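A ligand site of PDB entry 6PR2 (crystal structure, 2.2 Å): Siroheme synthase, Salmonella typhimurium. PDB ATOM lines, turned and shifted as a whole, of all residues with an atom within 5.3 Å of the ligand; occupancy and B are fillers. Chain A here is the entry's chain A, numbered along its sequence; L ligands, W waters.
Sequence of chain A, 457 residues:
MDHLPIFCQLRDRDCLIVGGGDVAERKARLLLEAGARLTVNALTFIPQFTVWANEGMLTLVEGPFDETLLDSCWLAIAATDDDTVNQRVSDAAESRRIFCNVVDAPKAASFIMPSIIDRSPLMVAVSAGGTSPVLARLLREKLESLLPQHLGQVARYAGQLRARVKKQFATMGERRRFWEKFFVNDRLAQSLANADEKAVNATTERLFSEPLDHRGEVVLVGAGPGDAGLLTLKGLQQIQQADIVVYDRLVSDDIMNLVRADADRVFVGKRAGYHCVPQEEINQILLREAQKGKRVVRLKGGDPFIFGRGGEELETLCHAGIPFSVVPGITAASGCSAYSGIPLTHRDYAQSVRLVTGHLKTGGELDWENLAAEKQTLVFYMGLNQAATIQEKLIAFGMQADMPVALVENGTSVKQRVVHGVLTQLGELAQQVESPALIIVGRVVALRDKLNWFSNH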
ATOM      1  N   PRO A 225     -23.514  12.672  -8.950  1.00  0.00           N
ATOM      2  CA  PRO A 225     -23.707  11.786 -10.098  1.00  0.00           C
ATOM      3  C   PRO A 225     -25.027  11.996 -10.832  1.00  0.00           C
ATOM      4  O   PRO A 225     -25.225  11.391 -11.893  1.00  0.00           O
ATOM      5  CB  PRO A 225     -23.642  10.389  -9.454  1.00  0.00           C
ATOM      6  CG  PRO A 225     -24.126  10.598  -8.096  1.00  0.00           C
ATOM      7  CD  PRO A 225     -23.788  12.016  -7.665  1.00  0.00           C
ATOM      8  N   GLY A 226     -25.906  12.852 -10.338  1.00  0.00           N
ATOM      9  CA  GLY A 226     -27.155  13.081 -11.053  1.00  0.00           C
ATOM     10  C   GLY A 226     -28.250  13.680 -10.200  1.00  0.00           C
ATOM     11  O   GLY A 226     -28.681  14.821 -10.441  1.00  0.00           O
ATOM     12  N   LEU A 250     -22.349  15.920 -18.285  1.00  0.00           N
ATOM     13  CA  LEU A 250     -22.476  15.025 -17.151  1.00  0.00           C
ATOM     14  C   LEU A 250     -22.928  15.732 -15.873  1.00  0.00           C
ATOM     15  O   LEU A 250     -22.796  15.179 -14.772  1.00  0.00           O
ATOM     16  CB  LEU A 250     -21.156  14.281 -16.916  1.00  0.00           C
ATOM     17  CG  LEU A 250     -21.011  13.087 -17.863  1.00  0.00           C
ATOM     18  CD1 LEU A 250     -19.788  12.239 -17.548  1.00  0.00           C
ATOM     19  CD2 LEU A 250     -22.286  12.240 -17.854  1.00  0.00           C
ATOM     20  N   GLY A 301     -19.517  16.799 -13.383  1.00  0.00           N
ATOM     21  CA  GLY A 301     -20.182  15.613 -12.863  1.00  0.00           C
ATOM     22  C   GLY A 301     -19.372  14.940 -11.781  1.00  0.00           C
ATOM     23  O   GLY A 301     -18.145  14.967 -11.781  1.00  0.00           O
ATOM     24  N   GLY A 302     -20.074  14.324 -10.812  1.00  0.00           N
ATOM     25  CA  GLY A 302     -19.430  13.498  -9.801  1.00  0.00           C
ATOM     26  C   GLY A 302     -18.518  14.330  -8.905  1.00  0.00           C
ATOM     27  O   GLY A 302     -18.927  15.365  -8.351  1.00  0.00           O
ATOM     28  N   ASP A 303     -17.263  13.872  -8.767  1.00  0.00           N
ATOM     29  CA  ASP A 303     -16.220  14.563  -8.004  1.00  0.00           C
ATOM     30  C   ASP A 303     -15.151  15.138  -8.935  1.00  0.00           C
ATOM     31  O   ASP A 303     -14.675  14.437  -9.840  1.00  0.00           O
ATOM     32  CB  ASP A 303     -15.569  13.596  -6.999  1.00  0.00           C
ATOM     33  CG  ASP A 303     -14.597  14.298  -6.043  1.00  0.00           C
ATOM     34  OD1 ASP A 303     -13.375  14.339  -6.344  1.00  0.00           O
ATOM     35  OD2 ASP A 303     -15.073  14.849  -5.010  1.00  0.00           O
ATOM     36  N   PRO A 304     -14.739  16.398  -8.741  1.00  0.00           N
ATOM     37  CA  PRO A 304     -13.800  17.036  -9.700  1.00  0.00           C
ATOM     38  C   PRO A 304     -12.436  16.387  -9.762  1.00  0.00           C
ATOM     39  O   PRO A 304     -11.754  16.526 -10.792  1.00  0.00           O
ATOM     40  CB  PRO A 304     -13.680  18.491  -9.201  1.00  0.00           C
ATOM     41  CG  PRO A 304     -14.775  18.683  -8.190  1.00  0.00           C
ATOM     42  CD  PRO A 304     -15.118  17.303  -7.634  1.00  0.00           C
ATOM     43  N   ILE A 306     -11.707  12.990  -9.340  1.00  0.00           N
ATOM     44  CA  ILE A 306     -11.714  11.568  -9.644  1.00  0.00           C
ATOM     45  C   ILE A 306     -12.063  11.446 -11.121  1.00  0.00           C
ATOM     46  O   ILE A 306     -13.223  11.607 -11.506  1.00  0.00           O
ATOM     47  CB  ILE A 306     -12.689  10.780  -8.763  1.00  0.00           C
ATOM     48  CG1 ILE A 306     -12.201  10.786  -7.306  1.00  0.00           C
ATOM     49  CG2 ILE A 306     -12.804   9.346  -9.267  1.00  0.00           C
ATOM     50  CD1 ILE A 306     -13.207  10.360  -6.282  1.00  0.00           C
ATOM     51  N   PHE A 307     -11.038  11.186 -11.950  1.00  0.00           N
ATOM     52  CA  PHE A 307     -11.195  11.072 -13.399  1.00  0.00           C
ATOM     53  C   PHE A 307     -11.911  12.300 -13.984  1.00  0.00           C
ATOM     54  O   PHE A 307     -12.626  12.204 -14.980  1.00  0.00           O
ATOM     55  CB  PHE A 307     -11.907   9.774 -13.779  1.00  0.00           C
ATOM     56  CG  PHE A 307     -11.229   8.544 -13.251  1.00  0.00           C
ATOM     57  CD1 PHE A 307      -9.894   8.298 -13.521  1.00  0.00           C
ATOM     58  CD2 PHE A 307     -11.914   7.637 -12.433  1.00  0.00           C
ATOM     59  CE1 PHE A 307      -9.246   7.164 -13.030  1.00  0.00           C
ATOM     60  CE2 PHE A 307     -11.293   6.491 -11.935  1.00  0.00           C
ATOM     61  CZ  PHE A 307      -9.957   6.259 -12.226  1.00  0.00           C
ATOM     62  N   GLY A 308     -11.727  13.456 -13.367  1.00  0.00           N
ATOM     63  CA  GLY A 308     -12.438  14.649 -13.781  1.00  0.00           C
ATOM     64  C   GLY A 308     -11.579  15.676 -14.506  1.00  0.00           C
ATOM     65  O   GLY A 308     -12.113  16.662 -15.014  1.00  0.00           O
ATOM     66  N   ILE A 330     -20.116  13.907  -4.636  1.00  0.00           N
ATOM     67  CA  ILE A 330     -20.341  12.462  -4.591  1.00  0.00           C
ATOM     68  C   ILE A 330     -19.825  11.863  -5.909  1.00  0.00           C
ATOM     69  O   ILE A 330     -20.382  12.134  -6.980  1.00  0.00           O
ATOM     70  CB  ILE A 330     -21.817  12.139  -4.383  1.00  0.00           C
ATOM     71  CG1 ILE A 330     -22.416  12.828  -3.133  1.00  0.00           C
ATOM     72  CG2 ILE A 330     -22.027  10.621  -4.457  1.00  0.00           C
ATOM     73  CD1 ILE A 330     -21.832  12.394  -1.840  1.00  0.00           C
ATOM     74  N   THR A 331     -18.801  11.030  -5.854  1.00  0.00           N
ATOM     75  CA  THR A 331     -18.346  10.388  -7.086  1.00  0.00           C
ATOM     76  C   THR A 331     -19.352   9.330  -7.549  1.00  0.00           C
ATOM     77  O   THR A 331     -20.181   8.831  -6.772  1.00  0.00           O
ATOM     78  CB  THR A 331     -16.944   9.773  -6.901  1.00  0.00           C
ATOM     79  OG1 THR A 331     -16.400   9.391  -8.182  1.00  0.00           O
ATOM     80  CG2 THR A 331     -17.046   8.585  -5.972  1.00  0.00           C
ATOM     81  N   ALA A 332     -19.308   9.024  -8.845  1.00  0.00           N
ATOM     82  CA  ALA A 332     -20.258   8.039  -9.380  1.00  0.00           C
ATOM     83  C   ALA A 332     -20.245   6.731  -8.590  1.00  0.00           C
ATOM     84  O   ALA A 332     -21.298   6.109  -8.375  1.00  0.00           O
ATOM     85  CB  ALA A 332     -19.960   7.794 -10.860  1.00  0.00           C
ATOM     86  N   ALA A 333     -19.065   6.261  -8.171  1.00  0.00           N
ATOM     87  CA  ALA A 333     -19.006   5.009  -7.416  1.00  0.00           C
ATOM     88  C   ALA A 333     -19.852   5.085  -6.144  1.00  0.00           C
ATOM     89  O   ALA A 333     -20.599   4.141  -5.841  1.00  0.00           O
ATOM     90  CB  ALA A 333     -17.560   4.656  -7.073  1.00  0.00           C
ATOM     91  N   CYS A 336     -23.809   5.489  -7.198  1.00  0.00           N
ATOM     92  CA  CYS A 336     -24.367   4.248  -7.749  1.00  0.00           C
ATOM     93  C   CYS A 336     -24.348   3.127  -6.718  1.00  0.00           C
ATOM     94  O   CYS A 336     -25.257   2.282  -6.688  1.00  0.00           O
ATOM     95  CB  CYS A 336     -23.586   3.812  -8.986  1.00  0.00           C
ATOM     96  SG  CYS A 336     -23.697   4.885 -10.458  1.00  0.00           S
ATOM     97  N   PHE A 380     -15.127   0.347 -12.640  1.00  0.00           N
ATOM     98  CA  PHE A 380     -14.577   0.869 -13.883  1.00  0.00           C
ATOM     99  C   PHE A 380     -15.394   2.082 -14.307  1.00  0.00           C
ATOM    100  O   PHE A 380     -16.608   1.991 -14.483  1.00  0.00           O
ATOM    101  CB  PHE A 380     -14.582  -0.171 -14.995  1.00  0.00           C
ATOM    102  CG  PHE A 380     -13.631  -1.314 -14.763  1.00  0.00           C
ATOM    103  CD1 PHE A 380     -12.334  -1.267 -15.241  1.00  0.00           C
ATOM    104  CD2 PHE A 380     -14.049  -2.443 -14.060  1.00  0.00           C
ATOM    105  CE1 PHE A 380     -11.450  -2.328 -15.022  1.00  0.00           C
ATOM    106  CE2 PHE A 380     -13.184  -3.516 -13.830  1.00  0.00           C
ATOM    107  CZ  PHE A 380     -11.883  -3.451 -14.292  1.00  0.00           C
ATOM    108  N   TYR A 381     -14.705   3.206 -14.465  1.00  0.00           N
ATOM    109  CA  TYR A 381     -15.250   4.419 -15.071  1.00  0.00           C
ATOM    110  C   TYR A 381     -14.931   4.428 -16.558  1.00  0.00           C
ATOM    111  O   TYR A 381     -13.848   3.999 -16.975  1.00  0.00           O
ATOM    112  CB  TYR A 381     -14.631   5.645 -14.407  1.00  0.00           C
ATOM    113  CG  TYR A 381     -15.105   5.967 -12.992  1.00  0.00           C
ATOM    114  CD1 TYR A 381     -14.813   5.115 -11.905  1.00  0.00           C
ATOM    115  CD2 TYR A 381     -15.787   7.153 -12.731  1.00  0.00           C
ATOM    116  CE1 TYR A 381     -15.220   5.443 -10.590  1.00  0.00           C
ATOM    117  CE2 TYR A 381     -16.212   7.492 -11.424  1.00  0.00           C
ATOM    118  CZ  TYR A 381     -15.928   6.634 -10.365  1.00  0.00           C
ATOM    119  OH  TYR A 381     -16.355   6.968  -9.096  1.00  0.00           O
ATOM    120  N   MET A 382     -15.883   4.918 -17.365  1.00  0.00           N
ATOM    121  CA  MET A 382     -15.706   5.030 -18.811  1.00  0.00           C
ATOM    122  C   MET A 382     -15.256   3.712 -19.433  1.00  0.00           C
ATOM    123  O   MET A 382     -14.307   3.678 -20.223  1.00  0.00           O
ATOM    124  CB  MET A 382     -14.684   6.109 -19.182  1.00  0.00           C
ATOM    125  CG  MET A 382     -14.850   7.464 -18.511  1.00  0.00           C
ATOM    126  SD  MET A 382     -13.275   8.350 -18.623  1.00  0.00           S
ATOM    127  CE  MET A 382     -12.471   7.769 -17.125  1.00  0.00           C
ATOM    128  N   GLY A 383     -15.901   2.608 -19.062  1.00  0.00           N
ATOM    129  CA  GLY A 383     -15.381   1.311 -19.478  1.00  0.00           C
ATOM    130  C   GLY A 383     -16.288   0.511 -20.378  1.00  0.00           C
ATOM    131  O   GLY A 383     -15.997  -0.642 -20.692  1.00  0.00           O
ATOM    132  N   VAL A 408     -24.297  -0.011 -13.736  1.00  0.00           N
ATOM    133  CA  VAL A 408     -25.268   0.974 -13.309  1.00  0.00           C
ATOM    134  C   VAL A 408     -25.261   2.103 -14.324  1.00  0.00           C
ATOM    135  O   VAL A 408     -24.231   2.771 -14.510  1.00  0.00           O
ATOM    136  CB  VAL A 408     -24.987   1.446 -11.874  1.00  0.00           C
ATOM    137  CG1 VAL A 408     -26.121   2.413 -11.403  1.00  0.00           C
ATOM    138  CG2 VAL A 408     -24.916   0.226 -10.991  1.00  0.00           C
ATOM    139  N   GLU A 409     -26.381   2.279 -15.009  1.00  0.00           N
ATOM    140  CA  GLU A 409     -26.535   3.313 -16.013  1.00  0.00           C
ATOM    141  C   GLU A 409     -27.344   4.459 -15.424  1.00  0.00           C
ATOM    142  O   GLU A 409     -28.425   4.241 -14.862  1.00  0.00           O
ATOM    143  CB  GLU A 409     -27.212   2.780 -17.275  1.00  0.00           C
ATOM    144  CG  GLU A 409     -27.285   3.830 -18.382  1.00  0.00           C
ATOM    145  CD  GLU A 409     -28.210   3.453 -19.551  1.00  0.00           C
ATOM    146  OE1 GLU A 409     -28.547   2.261 -19.727  1.00  0.00           O
ATOM    147  OE2 GLU A 409     -28.575   4.377 -20.310  1.00  0.00           O
ATOM    148  N   ASN A 410     -26.801   5.675 -15.534  1.00  0.00           N
ATOM    149  CA  ASN A 410     -27.499   6.867 -15.038  1.00  0.00           C
ATOM    150  C   ASN A 410     -27.794   6.716 -13.548  1.00  0.00           C
ATOM    151  O   ASN A 410     -28.922   6.948 -13.094  1.00  0.00           O
ATOM    152  CB  ASN A 410     -28.771   7.130 -15.852  1.00  0.00           C
ATOM    153  CG  ASN A 410     -28.466   7.689 -17.227  1.00  0.00           C
ATOM    154  OD1 ASN A 410     -27.661   8.617 -17.349  1.00  0.00           O
ATOM    155  ND2 ASN A 410     -29.072   7.115 -18.270  1.00  0.00           N
ATOM    156  N   GLY A 411     -26.769   6.327 -12.799  1.00  0.00           N
ATOM    157  CA  GLY A 411     -26.953   6.057 -11.381  1.00  0.00           C
ATOM    158  C   GLY A 411     -27.465   7.289 -10.658  1.00  0.00           C
ATOM    159  O   GLY A 411     -27.060   8.420 -10.963  1.00  0.00           O
ATOM    160  N   THR A 412     -28.379   7.068  -9.713  1.00  0.00           N
ATOM    161  CA  THR A 412     -29.049   8.030  -8.819  1.00  0.00           C
ATOM    162  C   THR A 412     -30.116   8.873  -9.499  1.00  0.00           C
ATOM    163  O   THR A 412     -30.793   9.621  -8.804  1.00  0.00           O
ATOM    164  CB  THR A 412     -28.104   9.008  -8.091  1.00  0.00           C
ATOM    165  OG1 THR A 412     -27.750  10.108  -8.950  1.00  0.00           O
ATOM    166  CG2 THR A 412     -26.836   8.316  -7.529  1.00  0.00           C
ATOM    167  N   PRO A 436     -23.970   7.392 -19.558  1.00  0.00           N
ATOM    168  CA  PRO A 436     -22.849   7.085 -18.662  1.00  0.00           C
ATOM    169  C   PRO A 436     -23.173   5.888 -17.766  1.00  0.00           C
ATOM    170  O   PRO A 436     -24.297   5.779 -17.257  1.00  0.00           O
ATOM    171  CB  PRO A 436     -22.703   8.371 -17.838  1.00  0.00           C
ATOM    172  CG  PRO A 436     -24.089   8.918 -17.770  1.00  0.00           C
ATOM    173  CD  PRO A 436     -24.747   8.556 -19.087  1.00  0.00           C
ATOM    174  N   ALA A 437     -22.212   4.988 -17.606  1.00  0.00           N
ATOM    175  CA  ALA A 437     -22.441   3.789 -16.819  1.00  0.00           C
ATOM    176  C   ALA A 437     -21.159   3.388 -16.101  1.00  0.00           C
ATOM    177  O   ALA A 437     -20.046   3.617 -16.597  1.00  0.00           O
ATOM    178  CB  ALA A 437     -22.930   2.636 -17.689  1.00  0.00           C
ATOM    179  N   LEU A 438     -21.320   2.781 -14.931  1.00  0.00           N
ATOM    180  CA  LEU A 438     -20.240   2.171 -14.185  1.00  0.00           C
ATOM    181  C   LEU A 438     -20.308   0.664 -14.327  1.00  0.00           C
ATOM    182  O   LEU A 438     -21.397   0.087 -14.415  1.00  0.00           O
ATOM    183  CB  LEU A 438     -20.319   2.508 -12.696  1.00  0.00           C
ATOM    184  CG  LEU A 438     -19.888   3.871 -12.232  1.00  0.00           C
ATOM    185  CD1 LEU A 438     -19.872   3.865 -10.730  1.00  0.00           C
ATOM    186  CD2 LEU A 438     -18.522   4.195 -12.802  1.00  0.00           C
HETATM  187  N1  LIG L   1     -15.642  12.943 -12.084  1.00  0.00           N
HETATM  188  C1  LIG L   1     -16.705  11.954 -12.267  1.00  0.00           C
HETATM  189  C2  LIG L   1     -16.306  10.908 -13.303  1.00  0.00           C
HETATM  190  C3  LIG L   1     -16.142  11.430 -14.717  1.00  0.00           C
HETATM  191  S1  LIG L   1     -15.439  10.165 -15.812  1.00  0.00           S
HETATM  192  C4  LIG L   1     -17.043  11.263 -10.954  1.00  0.00           C
HETATM  193  O1  LIG L   1     -16.438  11.545  -9.922  1.00  0.00           O
HETATM  194  O2  LIG L   1     -17.903  10.386 -10.913  1.00  0.00           O
HETATM  195  C5  LIG L   1     -17.011   9.766 -16.619  1.00  0.00           C
HETATM  196  C6  LIG L   1     -17.544   8.396 -16.215  1.00  0.00           C
HETATM  197  O3  LIG L   1     -18.132   8.431 -14.919  1.00  0.00           O
HETATM  198  C7  LIG L   1     -18.622   7.828 -17.129  1.00  0.00           C
HETATM  199  O4  LIG L   1     -18.088   7.148 -18.241  1.00  0.00           O
HETATM  200  C8  LIG L   1     -19.323   6.838 -16.229  1.00  0.00           C
HETATM  201  O5  LIG L   1     -18.584   5.635 -16.159  1.00  0.00           O
HETATM  202  C9  LIG L   1     -19.189   7.489 -14.860  1.00  0.00           C
HETATM  203  N2  LIG L   1     -20.419   8.133 -14.400  1.00  0.00           N
HETATM  204  C10 LIG L   1     -20.630   9.483 -14.184  1.00  0.00           C
HETATM  205  N3  LIG L   1     -21.913   9.657 -13.768  1.00  0.00           N
HETATM  206  C11 LIG L   1     -22.506   8.432 -13.735  1.00  0.00           C
HETATM  207  C12 LIG L   1     -23.787   8.028 -13.371  1.00  0.00           C
HETATM  208  N4  LIG L   1     -24.684   8.939 -12.984  1.00  0.00           N
HETATM  209  N5  LIG L   1     -24.116   6.695 -13.414  1.00  0.00           N
HETATM  210  C13 LIG L   1     -23.182   5.768 -13.830  1.00  0.00           C
HETATM  211  N6  LIG L   1     -21.906   6.171 -14.184  1.00  0.00           N
HETATM  212  C14 LIG L   1     -21.573   7.481 -14.131  1.00  0.00           C
HETATM  213  O   HOH W   1     -20.060   5.432 -19.684  1.00  0.00           O
HETATM  214  O   HOH W   2     -19.195  12.758 -14.541  1.00  0.00           O
HETATM  215  O   HOH W   3     -15.827  15.193 -13.463  1.00  0.00           O
HETATM  216  O   HOH W   4     -22.023  12.436 -13.149  1.00  0.00           O
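O of Pro 436 is in hydrogen-bond range of N of Asn 410 (3.0 Å). SG of Cys 336 sits close to O of Ala 332 (3.4 Å). The side-chain hydroxyl of Tyr 381 is in hydrogen-bond range of the backbone NH of Ala 333 (2.9 Å). The backbone carbonyl oxygen of Val 408 sits at hydrogen-bond distance from the backbone NH of Leu 438, at 2.9 Å. The side-chain carboxylate (OE2) of Glu 409 is in hydrogen-bond range of the side-chain amide nitrogen (ND2) of Asn 410. OG1 of Thr 331 sits at hydrogen-bond distance from OH of Tyr 381 (2.6 Å).
Water W3 bridges a nitrogen (N1) of the ligand (2.6 Å) and the backbone carbonyl oxygen of Gly 301 (2.9 Å). Water W4 bridges a nitrogen (N3) of the ligand (2.8 Å) and the backbone carbonyl oxygen of Leu 250 (3.3 Å). Water W1 lies within hydrogen-bond range of an oxygen (O4) of the ligand (3.0 Å) and the backbone NH of Ala 437 (3.0 Å).
The backbone carbonyl oxygen (O) of Gly 411 lies within hydrogen-bond range of a nitrogen (N4) of the ligand, 3.2 Å away. A nitrogen (N1) of the ligand is in hydrogen-bond range of the backbone carbonyl oxygen of Gly 301 (3.2 Å). The backbone carbonyl oxygen (O) of Asp 303 sits at hydrogen-bond distance from a nitrogen (N1) of the ligand (2.9 Å). N of Ala 332 lies within hydrogen-bond range of O2 of the ligand. The backbone carbonyl oxygen (O) of Pro 225 lies within hydrogen-bond range of a nitrogen (N4) of the ligand, 2.7 Å away. A nitrogen (N1) of the ligand sits at hydrogen-bond distance from the backbone carbonyl oxygen (O) of Ile 306. The side-chain hydroxyl of Thr 331 sits at hydrogen-bond distance from an oxygen (O1) of the ligand, at 2.8 Å. O1 of the ligand is in hydrogen-bond range of N of Asp 303. The backbone NH (N) of Met 382 sits at hydrogen-bond distance from an oxygen (O5) of the ligand. O of Ala 437 sits at hydrogen-bond distance from O5 of the ligand (2.5 Å). A nitrogen (N5) of the ligand lies within hydrogen-bond range of the side-chain sulfur (SG) of Cys 336, 3.5 Å away. The backbone NH of Gly 411 is in hydrogen-bond range of a nitrogen (N5) of the ligand (2.7 Å).
The backbone carbonyl oxygen of Phe 307 sits close to a sulfur (S1) of the ligand. Leu 250 touches the ligand. Gly 302 touches the ligand (CA to C4, 3.5 Å). Tyr 381 touches the ligand. Val 408 touches the ligand (O to C13, 3.2 Å). Asn 410 touches the ligand. Pro 436 touches the ligand (O to C13, 3.6 Å). Leu 438 touches the ligand (N to N6, 3.5 Å). Within 4 Å of the ligand: Pro 225, Leu 250, Gly 301, Gly 302, Asp 303, Ile 306, Phe 307, Thr 331, Ala 332, Cys 336, Tyr 381, Met 382, Val 408, Asn 410, Gly 411, Pro 436, Ala 437 and Leu 438. The nearest printed residue that does not touch the ligand is Gly 308 (4.01 Å).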
